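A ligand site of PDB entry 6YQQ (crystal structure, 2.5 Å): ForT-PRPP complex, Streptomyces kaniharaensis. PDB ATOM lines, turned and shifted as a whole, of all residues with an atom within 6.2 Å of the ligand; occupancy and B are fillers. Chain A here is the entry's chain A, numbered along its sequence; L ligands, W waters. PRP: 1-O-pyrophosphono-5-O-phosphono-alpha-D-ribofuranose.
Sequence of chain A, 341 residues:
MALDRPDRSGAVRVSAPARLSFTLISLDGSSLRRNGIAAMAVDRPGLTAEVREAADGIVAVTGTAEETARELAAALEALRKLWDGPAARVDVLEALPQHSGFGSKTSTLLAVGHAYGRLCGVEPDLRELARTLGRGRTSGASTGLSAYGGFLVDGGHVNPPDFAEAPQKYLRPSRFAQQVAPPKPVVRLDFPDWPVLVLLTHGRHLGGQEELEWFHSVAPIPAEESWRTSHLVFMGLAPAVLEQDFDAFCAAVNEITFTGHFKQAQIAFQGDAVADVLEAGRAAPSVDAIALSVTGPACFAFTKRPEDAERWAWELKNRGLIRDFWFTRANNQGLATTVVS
The side-chain hydroxyl (OG) of Ser 142 is in hydrogen-bond range of the guanidinium group (NH1) of Arg 19 (3.2 Å). N of Arg 19 is in hydrogen-bond range of O of Phe 102 (2.9 Å). The guanidinium group (NE) of Arg 135 is in hydrogen-bond range of the side-chain hydroxyl (OG1) of Thr 106 (3.1 Å). A ring nitrogen (NE2) of His 99 is in hydrogen-bond range of the side-chain carboxylate (OE2) of Glu 67 (3.0 Å). NZ of Lys 105 lies within salt-bridge range of OE2 of Glu 67 (3.2 Å). The backbone carbonyl oxygen (O) of Gly 103 lies within hydrogen-bond range of the side-chain hydroxyl (OG) of Ser 107, 2.7 Å away. The side-chain hydroxyl (OG) of Ser 293 sits at hydrogen-bond distance from the backbone carbonyl oxygen (O) of Gly 101, at 2.8 Å. OG of Ser 100 is in hydrogen-bond range of O of Gln 98 (3.0 Å).
Residues that only touch the ligand: Ser 100 (3.6 Å), Ala 141 (3.6 Å), Val 294 (3.7 Å) and Gln 98 (3.8 Å). 15 residues have an atom within 4 Å of the ligand: Arg 19, Gln 98, His 99, Ser 100, Gly 101, Phe 102, Gly 103, Ser 104, Lys 105, Thr 106, Arg 135, Ser 139, Ala 141, Ser 142 and Val 294.
Water W4 lies within hydrogen-bond range of an oxygen (O2P) of the ligand (2.6 Å), the side-chain hydroxyl (OG1) of Thr 106 (2.6 Å) and the guanidinium group (NH2) of Arg 135 (2.9 Å). Water W1 lies within hydrogen-bond range of OG1 of Thr 143, O of Ser 139 and O1P of the ligand. Water W3 lies within hydrogen-bond range of the backbone NH of Gly 296 and an oxygen (O2A) of the ligand.
An oxygen (O1A) of the ligand lies within salt-bridge range of the guanidinium group (NH2) of Arg 19 (2.5 Å). An oxygen (O1P) of the ligand sits at hydrogen-bond distance from the side-chain hydroxyl of Thr 106, at 2.6 Å. O1B of the ligand lies within hydrogen-bond range of N of Ser 104 (3.3 Å). OG of Ser 104 lies within hydrogen-bond range of O3B of the ligand (2.6 Å). An oxygen (O3P) of the ligand is in hydrogen-bond range of the side-chain hydroxyl (OG) of Ser 139 (2.6 Å). O3P of the ligand lies within hydrogen-bond range of N of Ser 142. The side-chain hydroxyl (OG) of Ser 142 sits at hydrogen-bond distance from an oxygen (O2P) of the ligand (2.8 Å). O3B of the ligand lies within hydrogen-bond range of N of His 99, 2.8 Å away. ND1 of His 99 sits at hydrogen-bond distance from O2B of the ligand (3.0 Å). The backbone NH (N) of Lys 105 is in hydrogen-bond range of an oxygen (O1B) of the ligand (2.9 Å). N of Gly 103 is in hydrogen-bond range of O1A of the ligand (3.2 Å). An oxygen (O2A) of the ligand is in hydrogen-bond range of the backbone NH of Gly 101 (3.2 Å). The backbone NH of Phe 102 sits at hydrogen-bond distance from an oxygen (O1A) of the ligand (3.4 Å). An oxygen (O1P) of the ligand lies within salt-bridge range of the guanidinium group (NH2) of Arg 135 (3.97 Å).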
ATOM      1  N   ARG A  19      22.007 -25.452  30.354  1.00  0.00           N
ATOM      2  CA  ARG A  19      22.109 -24.760  29.092  1.00  0.00           C
ATOM      3  C   ARG A  19      21.765 -23.311  29.365  1.00  0.00           C
ATOM      4  O   ARG A  19      20.686 -23.006  29.867  1.00  0.00           O
ATOM      5  CB  ARG A  19      21.111 -25.352  28.104  1.00  0.00           C
ATOM      6  CG  ARG A  19      21.206 -24.856  26.670  1.00  0.00           C
ATOM      7  CD  ARG A  19      20.558 -23.501  26.397  1.00  0.00           C
ATOM      8  NE  ARG A  19      19.337 -23.289  27.164  1.00  0.00           N
ATOM      9  CZ  ARG A  19      18.128 -23.697  26.807  1.00  0.00           C
ATOM     10  NH1 ARG A  19      17.928 -24.347  25.673  1.00  0.00           N
ATOM     11  NH2 ARG A  19      17.099 -23.425  27.587  1.00  0.00           N
ATOM     12  N   ILE A  37      20.192 -20.783  17.347  1.00  0.00           N
ATOM     13  CA  ILE A  37      20.441 -20.440  18.739  1.00  0.00           C
ATOM     14  C   ILE A  37      21.908 -20.597  19.097  1.00  0.00           C
ATOM     15  O   ILE A  37      22.501 -21.647  18.861  1.00  0.00           O
ATOM     16  CB  ILE A  37      19.609 -21.336  19.690  1.00  0.00           C
ATOM     17  CG1 ILE A  37      18.126 -21.170  19.365  1.00  0.00           C
ATOM     18  CG2 ILE A  37      19.901 -20.974  21.154  1.00  0.00           C
ATOM     19  CD1 ILE A  37      17.185 -21.783  20.378  1.00  0.00           C
ATOM     20  N   GLU A  67       5.448 -31.790  36.317  1.00  0.00           N
ATOM     21  CA  GLU A  67       5.483 -31.670  34.851  1.00  0.00           C
ATOM     22  C   GLU A  67       6.510 -32.610  34.191  1.00  0.00           C
ATOM     23  O   GLU A  67       6.147 -33.413  33.330  1.00  0.00           O
ATOM     24  CB  GLU A  67       5.750 -30.220  34.421  1.00  0.00           C
ATOM     25  CG  GLU A  67       5.816 -30.004  32.910  1.00  0.00           C
ATOM     26  CD  GLU A  67       5.899 -28.538  32.512  1.00  0.00           C
ATOM     27  OE1 GLU A  67       5.143 -27.718  33.076  1.00  0.00           O
ATOM     28  OE2 GLU A  67       6.698 -28.202  31.621  1.00  0.00           O
ATOM     29  N   LEU A  96      17.471 -29.706  37.750  1.00  0.00           N
ATOM     30  CA  LEU A  96      17.754 -28.415  37.140  1.00  0.00           C
ATOM     31  C   LEU A  96      16.532 -27.516  37.319  1.00  0.00           C
ATOM     32  O   LEU A  96      15.414 -27.955  37.054  1.00  0.00           O
ATOM     33  CB  LEU A  96      18.040 -28.578  35.659  1.00  0.00           C
ATOM     34  CG  LEU A  96      19.364 -29.252  35.345  1.00  0.00           C
ATOM     35  CD1 LEU A  96      19.328 -29.836  33.951  1.00  0.00           C
ATOM     36  CD2 LEU A  96      20.509 -28.257  35.487  1.00  0.00           C
ATOM     37  N   PRO A  97      16.677 -26.256  37.786  1.00  0.00           N
ATOM     38  CA  PRO A  97      15.517 -25.399  38.013  1.00  0.00           C
ATOM     39  C   PRO A  97      14.639 -25.264  36.768  1.00  0.00           C
ATOM     40  O   PRO A  97      15.125 -24.934  35.682  1.00  0.00           O
ATOM     41  CB  PRO A  97      16.134 -24.052  38.421  1.00  0.00           C
ATOM     42  CG  PRO A  97      17.513 -24.392  38.894  1.00  0.00           C
ATOM     43  CD  PRO A  97      17.948 -25.603  38.118  1.00  0.00           C
ATOM     44  N   GLN A  98      13.342 -25.543  36.938  1.00  0.00           N
ATOM     45  CA  GLN A  98      12.389 -25.653  35.854  1.00  0.00           C
ATOM     46  C   GLN A  98      11.913 -24.280  35.371  1.00  0.00           C
ATOM     47  O   GLN A  98      11.666 -23.389  36.183  1.00  0.00           O
ATOM     48  CB  GLN A  98      11.185 -26.485  36.329  1.00  0.00           C
ATOM     49  CG  GLN A  98      10.313 -27.026  35.216  1.00  0.00           C
ATOM     50  CD  GLN A  98       9.105 -27.787  35.740  1.00  0.00           C
ATOM     51  OE1 GLN A  98       8.481 -27.367  36.714  1.00  0.00           O
ATOM     52  NE2 GLN A  98       8.789 -28.894  35.093  1.00  0.00           N
ATOM     53  N   HIS A  99      11.800 -24.127  34.045  1.00  0.00           N
ATOM     54  CA  HIS A  99      11.339 -22.890  33.384  1.00  0.00           C
ATOM     55  C   HIS A  99      12.044 -21.650  33.916  1.00  0.00           C
ATOM     56  O   HIS A  99      11.429 -20.595  34.100  1.00  0.00           O
ATOM     57  CB  HIS A  99       9.814 -22.722  33.518  1.00  0.00           C
ATOM     58  CG  HIS A  99       9.012 -23.881  33.018  1.00  0.00           C
ATOM     59  ND1 HIS A  99       9.240 -24.470  31.790  1.00  0.00           N
ATOM     60  CD2 HIS A  99       7.990 -24.576  33.586  1.00  0.00           C
ATOM     61  CE1 HIS A  99       8.399 -25.471  31.618  1.00  0.00           C
ATOM     62  NE2 HIS A  99       7.626 -25.557  32.688  1.00  0.00           N
ATOM     63  N   SER A 100      13.352 -21.785  34.166  1.00  0.00           N
ATOM     64  CA  SER A 100      14.170 -20.709  34.697  1.00  0.00           C
ATOM     65  C   SER A 100      15.261 -20.255  33.740  1.00  0.00           C
ATOM     66  O   SER A 100      16.120 -19.453  34.110  1.00  0.00           O
ATOM     67  CB  SER A 100      14.809 -21.147  36.018  1.00  0.00           C
ATOM     68  OG  SER A 100      13.799 -21.458  36.965  1.00  0.00           O
ATOM     69  N   GLY A 101      15.209 -20.763  32.494  1.00  0.00           N
ATOM     70  CA  GLY A 101      16.171 -20.418  31.466  1.00  0.00           C
ATOM     71  C   GLY A 101      17.423 -21.280  31.507  1.00  0.00           C
ATOM     72  O   GLY A 101      18.497 -20.804  31.117  1.00  0.00           O
ATOM     73  N   PHE A 102      17.280 -22.533  31.951  1.00  0.00           N
ATOM     74  CA  PHE A 102      18.391 -23.504  32.056  1.00  0.00           C
ATOM     75  C   PHE A 102      18.281 -24.725  31.137  1.00  0.00           C
ATOM     76  O   PHE A 102      19.171 -25.576  31.130  1.00  0.00           O
ATOM     77  CB  PHE A 102      18.549 -23.977  33.515  1.00  0.00           C
ATOM     78  CG  PHE A 102      19.035 -22.898  34.458  1.00  0.00           C
ATOM     79  CD1 PHE A 102      20.228 -22.238  34.220  1.00  0.00           C
ATOM     80  CD2 PHE A 102      18.291 -22.550  35.586  1.00  0.00           C
ATOM     81  CE1 PHE A 102      20.676 -21.253  35.087  1.00  0.00           C
ATOM     82  CE2 PHE A 102      18.729 -21.562  36.454  1.00  0.00           C
ATOM     83  CZ  PHE A 102      19.926 -20.917  36.211  1.00  0.00           C
ATOM     84  N   GLY A 103      17.198 -24.811  30.356  1.00  0.00           N
ATOM     85  CA  GLY A 103      16.955 -25.934  29.458  1.00  0.00           C
ATOM     86  C   GLY A 103      16.830 -27.251  30.188  1.00  0.00           C
ATOM     87  O   GLY A 103      17.478 -28.235  29.814  1.00  0.00           O
ATOM     88  N   SER A 104      15.988 -27.284  31.228  1.00  0.00           N
ATOM     89  CA  SER A 104      15.881 -28.406  32.139  1.00  0.00           C
ATOM     90  C   SER A 104      15.198 -29.632  31.553  1.00  0.00           C
ATOM     91  O   SER A 104      15.606 -30.759  31.806  1.00  0.00           O
ATOM     92  CB  SER A 104      15.160 -27.991  33.423  1.00  0.00           C
ATOM     93  OG  SER A 104      13.822 -27.603  33.153  1.00  0.00           O
ATOM     94  N   LYS A 105      14.136 -29.416  30.766  1.00  0.00           N
ATOM     95  CA  LYS A 105      13.328 -30.531  30.282  1.00  0.00           C
ATOM     96  C   LYS A 105      14.125 -31.363  29.285  1.00  0.00           C
ATOM     97  O   LYS A 105      14.373 -32.551  29.520  1.00  0.00           O
ATOM     98  CB  LYS A 105      11.986 -30.068  29.706  1.00  0.00           C
ATOM     99  CG  LYS A 105      10.906 -29.970  30.788  1.00  0.00           C
ATOM    100  CD  LYS A 105       9.878 -28.880  30.528  1.00  0.00           C
ATOM    101  CE  LYS A 105       8.995 -29.162  29.323  1.00  0.00           C
ATOM    102  NZ  LYS A 105       7.979 -30.227  29.556  1.00  0.00           N
ATOM    103  N   THR A 106      14.568 -30.732  28.195  1.00  0.00           N
ATOM    104  CA  THR A 106      15.403 -31.393  27.197  1.00  0.00           C
ATOM    105  C   THR A 106      16.564 -32.123  27.865  1.00  0.00           C
ATOM    106  O   THR A 106      16.779 -33.304  27.609  1.00  0.00           O
ATOM    107  CB  THR A 106      15.933 -30.377  26.174  1.00  0.00           C
ATOM    108  OG1 THR A 106      14.840 -29.606  25.661  1.00  0.00           O
ATOM    109  CG2 THR A 106      16.646 -31.083  25.022  1.00  0.00           C
ATOM    110  N   SER A 107      17.287 -31.415  28.743  1.00  0.00           N
ATOM    111  CA  SER A 107      18.519 -31.898  29.350  1.00  0.00           C
ATOM    112  C   SER A 107      18.330 -33.105  30.269  1.00  0.00           C
ATOM    113  O   SER A 107      19.101 -34.073  30.204  1.00  0.00           O
ATOM    114  CB  SER A 107      19.223 -30.765  30.092  1.00  0.00           C
ATOM    115  OG  SER A 107      19.614 -29.744  29.183  1.00  0.00           O
ATOM    116  N   ARG A 135      11.388 -33.573  21.830  1.00  0.00           N
ATOM    117  CA  ARG A 135      12.192 -32.409  22.174  1.00  0.00           C
ATOM    118  C   ARG A 135      13.004 -31.886  20.983  1.00  0.00           C
ATOM    119  O   ARG A 135      13.247 -32.603  20.003  1.00  0.00           O
ATOM    120  CB  ARG A 135      13.142 -32.718  23.342  1.00  0.00           C
ATOM    121  CG  ARG A 135      12.458 -33.167  24.630  1.00  0.00           C
ATOM    122  CD  ARG A 135      11.436 -32.157  25.150  1.00  0.00           C
ATOM    123  NE  ARG A 135      12.003 -30.822  25.353  1.00  0.00           N
ATOM    124  CZ  ARG A 135      11.298 -29.758  25.740  1.00  0.00           C
ATOM    125  NH1 ARG A 135       9.996 -29.851  25.956  1.00  0.00           N
ATOM    126  NH2 ARG A 135      11.901 -28.586  25.892  1.00  0.00           N
ATOM    127  N   GLY A 136      13.415 -30.616  21.092  1.00  0.00           N
ATOM    128  CA  GLY A 136      14.240 -29.944  20.102  1.00  0.00           C
ATOM    129  C   GLY A 136      13.556 -29.721  18.759  1.00  0.00           C
ATOM    130  O   GLY A 136      14.145 -30.013  17.717  1.00  0.00           O
ATOM    131  N   ARG A 137      12.332 -29.191  18.791  1.00  0.00           N
ATOM    132  CA  ARG A 137      11.593 -28.845  17.574  1.00  0.00           C
ATOM    133  C   ARG A 137      11.727 -27.359  17.202  1.00  0.00           C
ATOM    134  O   ARG A 137      11.201 -26.930  16.180  1.00  0.00           O
ATOM    135  CB  ARG A 137      10.121 -29.227  17.724  1.00  0.00           C
ATOM    136  CG  ARG A 137       9.884 -30.678  18.125  1.00  0.00           C
ATOM    137  CD  ARG A 137       8.438 -31.100  17.945  1.00  0.00           C
ATOM    138  NE  ARG A 137       7.485 -30.149  18.530  1.00  0.00           N
ATOM    139  CZ  ARG A 137       6.860 -29.168  17.876  1.00  0.00           C
ATOM    140  NH1 ARG A 137       7.041 -28.968  16.578  1.00  0.00           N
ATOM    141  NH2 ARG A 137       6.024 -28.380  18.536  1.00  0.00           N
ATOM    142  N   THR A 138      12.415 -26.595  18.054  1.00  0.00           N
ATOM    143  CA  THR A 138      12.808 -25.210  17.789  1.00  0.00           C
ATOM    144  C   THR A 138      14.326 -25.081  17.886  1.00  0.00           C
ATOM    145  O   THR A 138      14.966 -24.504  17.008  1.00  0.00           O
ATOM    146  CB  THR A 138      12.179 -24.239  18.803  1.00  0.00           C
ATOM    147  OG1 THR A 138      10.751 -24.370  18.786  1.00  0.00           O
ATOM    148  CG2 THR A 138      12.546 -22.794  18.476  1.00  0.00           C
ATOM    149  N   SER A 139      14.884 -25.614  18.977  1.00  0.00           N
ATOM    150  CA  SER A 139      16.284 -25.449  19.338  1.00  0.00           C
ATOM    151  C   SER A 139      17.043 -26.761  19.316  1.00  0.00           C
ATOM    152  O   SER A 139      16.508 -27.793  19.720  1.00  0.00           O
ATOM    153  CB  SER A 139      16.369 -24.912  20.763  1.00  0.00           C
ATOM    154  OG  SER A 139      15.939 -25.896  21.676  1.00  0.00           O
ATOM    155  N   GLY A 140      18.297 -26.702  18.872  1.00  0.00           N
ATOM    156  CA  GLY A 140      19.253 -27.786  19.001  1.00  0.00           C
ATOM    157  C   GLY A 140      20.185 -27.571  20.168  1.00  0.00           C
ATOM    158  O   GLY A 140      21.059 -28.398  20.419  1.00  0.00           O
ATOM    159  N   ALA A 141      19.984 -26.470  20.895  1.00  0.00           N
ATOM    160  CA  ALA A 141      20.863 -26.025  21.979  1.00  0.00           C
ATOM    161  C   ALA A 141      21.149 -27.111  23.012  1.00  0.00           C
ATOM    162  O   ALA A 141      22.277 -27.580  23.118  1.00  0.00           O
ATOM    163  CB  ALA A 141      20.293 -24.786  22.651  1.00  0.00           C
ATOM    164  N   SER A 142      20.116 -27.510  23.758  1.00  0.00           N
ATOM    165  CA  SER A 142      20.259 -28.471  24.859  1.00  0.00           C
ATOM    166  C   SER A 142      20.589 -29.884  24.364  1.00  0.00           C
ATOM    167  O   SER A 142      21.283 -30.644  25.045  1.00  0.00           O
ATOM    168  CB  SER A 142      18.992 -28.498  25.723  1.00  0.00           C
ATOM    169  OG  SER A 142      18.879 -27.312  26.517  1.00  0.00           O
ATOM    170  N   THR A 143      20.079 -30.227  23.182  1.00  0.00           N
ATOM    171  CA  THR A 143      20.355 -31.525  22.553  1.00  0.00           C
ATOM    172  C   THR A 143      21.831 -31.600  22.170  1.00  0.00           C
ATOM    173  O   THR A 143      22.532 -32.550  22.530  1.00  0.00           O
ATOM    174  CB  THR A 143      19.470 -31.744  21.311  1.00  0.00           C
ATOM    175  OG1 THR A 143      18.122 -31.379  21.614  1.00  0.00           O
ATOM    176  CG2 THR A 143      19.512 -33.204  20.886  1.00  0.00           C
ATOM    177  N   SER A 293      19.135 -15.292  29.906  1.00  0.00           N
ATOM    178  CA  SER A 293      19.001 -16.617  29.309  1.00  0.00           C
ATOM    179  C   SER A 293      17.533 -16.893  28.986  1.00  0.00           C
ATOM    180  O   SER A 293      16.728 -17.127  29.891  1.00  0.00           O
ATOM    181  CB  SER A 293      19.591 -17.692  30.229  1.00  0.00           C
ATOM    182  OG  SER A 293      19.771 -18.915  29.523  1.00  0.00           O
ATOM    183  N   VAL A 294      17.203 -16.850  27.695  1.00  0.00           N
ATOM    184  CA  VAL A 294      15.840 -16.948  27.210  1.00  0.00           C
ATOM    185  C   VAL A 294      15.072 -15.746  27.818  1.00  0.00           C
ATOM    186  O   VAL A 294      15.451 -14.590  27.595  1.00  0.00           O
ATOM    187  CB  VAL A 294      15.206 -18.330  27.514  1.00  0.00           C
ATOM    188  CG1 VAL A 294      13.987 -18.573  26.628  1.00  0.00           C
ATOM    189  CG2 VAL A 294      16.215 -19.444  27.325  1.00  0.00           C
ATOM    190  N   GLY A 296      13.719 -16.630  31.154  1.00  0.00           N
ATOM    191  CA  GLY A 296      13.662 -17.180  32.503  1.00  0.00           C
ATOM    192  C   GLY A 296      14.549 -16.346  33.416  1.00  0.00           C
ATOM    193  O   GLY A 296      15.459 -15.686  32.942  1.00  0.00           O
HETATM  194  C1  PRP L   1      13.494 -23.324  26.848  1.00  0.00           C
HETATM  195  C2  PRP L   1      13.128 -22.231  25.851  1.00  0.00           C
HETATM  196  C3  PRP L   1      13.121 -22.955  24.519  1.00  0.00           C
HETATM  197  C4  PRP L   1      12.807 -24.405  24.871  1.00  0.00           C
HETATM  198  C5  PRP L   1      13.666 -25.410  24.108  1.00  0.00           C
HETATM  199  O1  PRP L   1      12.987 -23.063  28.170  1.00  0.00           O
HETATM  200  O2  PRP L   1      11.853 -21.654  26.140  1.00  0.00           O
HETATM  201  O3  PRP L   1      12.150 -22.397  23.617  1.00  0.00           O
HETATM  202  O4  PRP L   1      12.993 -24.549  26.288  1.00  0.00           O
HETATM  203  O5  PRP L   1      15.027 -25.366  24.527  1.00  0.00           O
HETATM  204  P   PRP L   1      15.986 -26.677  24.616  1.00  0.00           P
HETATM  205  O1P PRP L   1      15.241 -27.782  23.905  1.00  0.00           O
HETATM  206  O2P PRP L   1      16.169 -26.903  26.101  1.00  0.00           O
HETATM  207  O3P PRP L   1      17.249 -26.237  23.914  1.00  0.00           O
HETATM  208  PA  PRP L   1      13.917 -23.096  29.495  1.00  0.00           P
HETATM  209  O1A PRP L   1      15.296 -22.578  29.155  1.00  0.00           O
HETATM  210  O2A PRP L   1      13.177 -22.432  30.636  1.00  0.00           O
HETATM  211  O3A PRP L   1      14.036 -24.670  29.826  1.00  0.00           O
HETATM  212  PB  PRP L   1      12.822 -25.526  30.435  1.00  0.00           P
HETATM  213  O1B PRP L   1      13.007 -26.912  29.850  1.00  0.00           O
HETATM  214  O2B PRP L   1      11.583 -24.813  29.945  1.00  0.00           O
HETATM  215  O3B PRP L   1      13.034 -25.460  31.926  1.00  0.00           O
HETATM  216  O   HOH W   1      17.494 -29.053  21.941  1.00  0.00           O
HETATM  217  O   HOH W   2      15.035 -23.971  33.193  1.00  0.00           O
HETATM  218  O   HOH W   3      12.827 -19.018  30.217  1.00  0.00           O
HETATM  219  O   HOH W   4      14.201 -27.828  27.515  1.00  0.00           O
